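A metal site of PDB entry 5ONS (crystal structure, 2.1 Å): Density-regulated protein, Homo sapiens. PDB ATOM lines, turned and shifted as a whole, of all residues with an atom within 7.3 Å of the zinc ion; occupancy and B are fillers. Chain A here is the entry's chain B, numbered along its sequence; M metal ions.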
ATOM      1  N   TYR A  17       5.331 -26.262 -29.486  1.00  0.00           N
ATOM      2  CA  TYR A  17       4.150 -26.104 -28.649  1.00  0.00           C
ATOM      3  C   TYR A  17       4.569 -26.044 -27.188  1.00  0.00           C
ATOM      4  O   TYR A  17       5.300 -26.920 -26.698  1.00  0.00           O
ATOM      5  CB  TYR A  17       3.152 -27.245 -28.894  1.00  0.00           C
ATOM      6  CG  TYR A  17       2.567 -27.230 -30.311  1.00  0.00           C
ATOM      7  CD1 TYR A  17       1.818 -26.149 -30.758  1.00  0.00           C
ATOM      8  CD2 TYR A  17       2.770 -28.288 -31.170  1.00  0.00           C
ATOM      9  CE1 TYR A  17       1.294 -26.122 -32.028  1.00  0.00           C
ATOM     10  CE2 TYR A  17       2.236 -28.288 -32.448  1.00  0.00           C
ATOM     11  CZ  TYR A  17       1.497 -27.206 -32.873  1.00  0.00           C
ATOM     12  OH  TYR A  17       0.974 -27.203 -34.138  1.00  0.00           O
ATOM     13  N   CYS A  18       4.096 -25.009 -26.508  1.00  0.00           N
ATOM     14  CA  CYS A  18       4.451 -24.770 -25.120  1.00  0.00           C
ATOM     15  C   CYS A  18       4.102 -25.968 -24.238  1.00  0.00           C
ATOM     16  O   CYS A  18       3.035 -26.570 -24.372  1.00  0.00           O
ATOM     17  CB  CYS A  18       3.732 -23.516 -24.643  1.00  0.00           C
ATOM     18  SG  CYS A  18       3.749 -23.358 -22.815  1.00  0.00           S
ATOM     19  N   GLY A  19       5.015 -26.310 -23.333  1.00  0.00           N
ATOM     20  CA  GLY A  19       4.868 -27.500 -22.523  1.00  0.00           C
ATOM     21  C   GLY A  19       3.824 -27.398 -21.441  1.00  0.00           C
ATOM     22  O   GLY A  19       3.430 -28.432 -20.881  1.00  0.00           O
ATOM     23  N   VAL A  20       3.357 -26.185 -21.124  1.00  0.00           N
ATOM     24  CA  VAL A  20       2.313 -26.064 -20.110  1.00  0.00           C
ATOM     25  C   VAL A  20       0.928 -25.833 -20.715  1.00  0.00           C
ATOM     26  O   VAL A  20       0.025 -26.651 -20.502  1.00  0.00           O
ATOM     27  CB  VAL A  20       2.687 -25.016 -19.025  1.00  0.00           C
ATOM     28  CG1 VAL A  20       3.200 -23.720 -19.612  1.00  0.00           C
ATOM     29  CG2 VAL A  20       1.526 -24.792 -18.057  1.00  0.00           C
ATOM     30  N   CYS A  21       0.746 -24.791 -21.533  1.00  0.00           N
ATOM     31  CA  CYS A  21      -0.595 -24.604 -22.080  1.00  0.00           C
ATOM     32  C   CYS A  21      -0.822 -25.345 -23.396  1.00  0.00           C
ATOM     33  O   CYS A  21      -1.960 -25.367 -23.877  1.00  0.00           O
ATOM     34  CB  CYS A  21      -0.891 -23.115 -22.276  1.00  0.00           C
ATOM     35  SG  CYS A  21      -0.015 -22.396 -23.685  1.00  0.00           S
ATOM     36  N   SER A  22       0.221 -25.921 -24.015  1.00  0.00           N
ATOM     37  CA  SER A  22       0.170 -26.723 -25.237  1.00  0.00           C
ATOM     38  C   SER A  22      -0.034 -25.907 -26.522  1.00  0.00           C
ATOM     39  O   SER A  22      -0.179 -26.492 -27.595  1.00  0.00           O
ATOM     40  CB  SER A  22      -0.908 -27.811 -25.202  1.00  0.00           C
ATOM     41  OG  SER A  22      -2.126 -27.319 -25.745  1.00  0.00           O
ATOM     42  N   LEU A  23      -0.049 -24.594 -26.438  1.00  0.00           N
ATOM     43  CA  LEU A  23      -0.253 -23.673 -27.545  1.00  0.00           C
ATOM     44  C   LEU A  23       1.072 -23.258 -28.170  1.00  0.00           C
ATOM     45  O   LEU A  23       2.129 -23.443 -27.551  1.00  0.00           O
ATOM     46  CB  LEU A  23      -1.005 -22.444 -27.048  1.00  0.00           C
ATOM     47  CG  LEU A  23      -2.527 -22.576 -27.040  1.00  0.00           C
ATOM     48  CD1 LEU A  23      -2.988 -23.908 -26.474  1.00  0.00           C
ATOM     49  CD2 LEU A  23      -3.092 -21.456 -26.220  1.00  0.00           C
ATOM     50  N   PRO A  24       1.057 -22.741 -29.402  1.00  0.00           N
ATOM     51  CA  PRO A  24       2.251 -22.045 -29.901  1.00  0.00           C
ATOM     52  C   PRO A  24       2.617 -20.927 -28.936  1.00  0.00           C
ATOM     53  O   PRO A  24       1.742 -20.243 -28.424  1.00  0.00           O
ATOM     54  CB  PRO A  24       1.810 -21.504 -31.262  1.00  0.00           C
ATOM     55  CG  PRO A  24       0.682 -22.401 -31.679  1.00  0.00           C
ATOM     56  CD  PRO A  24      -0.028 -22.729 -30.396  1.00  0.00           C
ATOM     57  N   THR A  25       3.921 -20.763 -28.678  1.00  0.00           N
ATOM     58  CA  THR A  25       4.372 -19.901 -27.592  1.00  0.00           C
ATOM     59  C   THR A  25       3.966 -18.445 -27.791  1.00  0.00           C
ATOM     60  O   THR A  25       4.061 -17.653 -26.834  1.00  0.00           O
ATOM     61  CB  THR A  25       5.893 -19.983 -27.389  1.00  0.00           C
ATOM     62  OG1 THR A  25       6.576 -19.661 -28.615  1.00  0.00           O
ATOM     63  CG2 THR A  25       6.309 -21.375 -26.916  1.00  0.00           C
ATOM     64  N   GLU A  26       3.514 -18.069 -28.984  1.00  0.00           N
ATOM     65  CA  GLU A  26       2.973 -16.744 -29.242  1.00  0.00           C
ATOM     66  C   GLU A  26       1.543 -16.577 -28.730  1.00  0.00           C
ATOM     67  O   GLU A  26       1.036 -15.452 -28.717  1.00  0.00           O
ATOM     68  CB  GLU A  26       3.016 -16.441 -30.741  1.00  0.00           C
ATOM     69  CG  GLU A  26       2.030 -17.253 -31.542  1.00  0.00           C
ATOM     70  CD  GLU A  26       2.260 -17.156 -33.040  1.00  0.00           C
ATOM     71  OE1 GLU A  26       1.753 -18.028 -33.774  1.00  0.00           O
ATOM     72  OE2 GLU A  26       2.938 -16.205 -33.494  1.00  0.00           O
ATOM     73  N   TYR A  27       0.886 -17.671 -28.345  1.00  0.00           N
ATOM     74  CA  TYR A  27      -0.450 -17.634 -27.734  1.00  0.00           C
ATOM     75  C   TYR A  27      -0.444 -17.868 -26.233  1.00  0.00           C
ATOM     76  O   TYR A  27      -1.516 -17.791 -25.616  1.00  0.00           O
ATOM     77  CB  TYR A  27      -1.370 -18.665 -28.399  1.00  0.00           C
ATOM     78  CG  TYR A  27      -1.702 -18.263 -29.806  1.00  0.00           C
ATOM     79  CD1 TYR A  27      -2.607 -17.247 -30.042  1.00  0.00           C
ATOM     80  CD2 TYR A  27      -1.071 -18.856 -30.903  1.00  0.00           C
ATOM     81  CE1 TYR A  27      -2.921 -16.834 -31.320  1.00  0.00           C
ATOM     82  CE2 TYR A  27      -1.378 -18.458 -32.214  1.00  0.00           C
ATOM     83  CZ  TYR A  27      -2.305 -17.436 -32.400  1.00  0.00           C
ATOM     84  OH  TYR A  27      -2.637 -16.987 -33.662  1.00  0.00           O
ATOM     85  N   CYS A  28       0.717 -18.175 -25.637  1.00  0.00           N
ATOM     86  CA  CYS A  28       0.830 -18.285 -24.175  1.00  0.00           C
ATOM     87  C   CYS A  28       0.137 -17.124 -23.478  1.00  0.00           C
ATOM     88  O   CYS A  28      -0.574 -17.304 -22.483  1.00  0.00           O
ATOM     89  CB  CYS A  28       2.303 -18.326 -23.774  1.00  0.00           C
ATOM     90  SG  CYS A  28       3.163 -19.851 -24.114  1.00  0.00           S
ATOM     91  N   GLU A  29       0.353 -15.911 -23.993  1.00  0.00           N
ATOM     92  CA  GLU A  29      -0.243 -14.672 -23.513  1.00  0.00           C
ATOM     93  C   GLU A  29      -1.714 -14.811 -23.116  1.00  0.00           C
ATOM     94  O   GLU A  29      -2.180 -14.105 -22.219  1.00  0.00           O
ATOM     95  CB  GLU A  29      -0.099 -13.611 -24.611  1.00  0.00           C
ATOM     96  CG  GLU A  29       1.112 -12.754 -24.440  1.00  0.00           C
ATOM     97  CD  GLU A  29       1.190 -11.689 -25.504  1.00  0.00           C
ATOM     98  OE1 GLU A  29       1.520 -10.533 -25.177  1.00  0.00           O
ATOM     99  OE2 GLU A  29       0.932 -12.034 -26.685  1.00  0.00           O
ATOM    100  N   MET A  31      -3.352 -17.719 -22.141  1.00  0.00           N
ATOM    101  CA  MET A  31      -3.668 -18.867 -21.285  1.00  0.00           C
ATOM    102  C   MET A  31      -3.098 -18.681 -19.887  1.00  0.00           C
ATOM    103  O   MET A  31      -1.857 -18.713 -19.714  1.00  0.00           O
ATOM    104  CB  MET A  31      -3.140 -20.160 -21.911  1.00  0.00           C
ATOM    105  CG  MET A  31      -3.645 -20.374 -23.337  1.00  0.00           C
ATOM    106  SD  MET A  31      -5.198 -21.297 -23.469  1.00  0.00           S
ATOM    107  CE  MET A  31      -6.253 -20.189 -24.420  1.00  0.00           C
HETATM  108 ZN    ZN M   1       2.061 -21.693 -22.895  1.00  0.00          ZN
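The zinc ion is bound by the side-chain sulfur of Cys 21 (2.3 Å), the side-chain sulfur of Cys 18 (2.4 Å) and the side-chain sulfur of Cys 28 (2.5 Å). The zinc ion has three donor atoms within binding distance.
Of the 14 residues printed, 3 come within 4 Å of the zinc ion.
N of Leu 23 lies close to SG of Cys 21, 3.5 Å away. The side-chain sulfur (SG) of Cys 18 sits close to the backbone NH (N) of Val 20. The backbone NH (N) of Cys 18 sits at hydrogen-bond distance from the backbone carbonyl oxygen (O) of Leu 23 (2.7 Å). The side-chain sulfur (SG) of Cys 28 lies close to the backbone carbonyl oxygen (O) of Thr 25 (3.6 Å).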
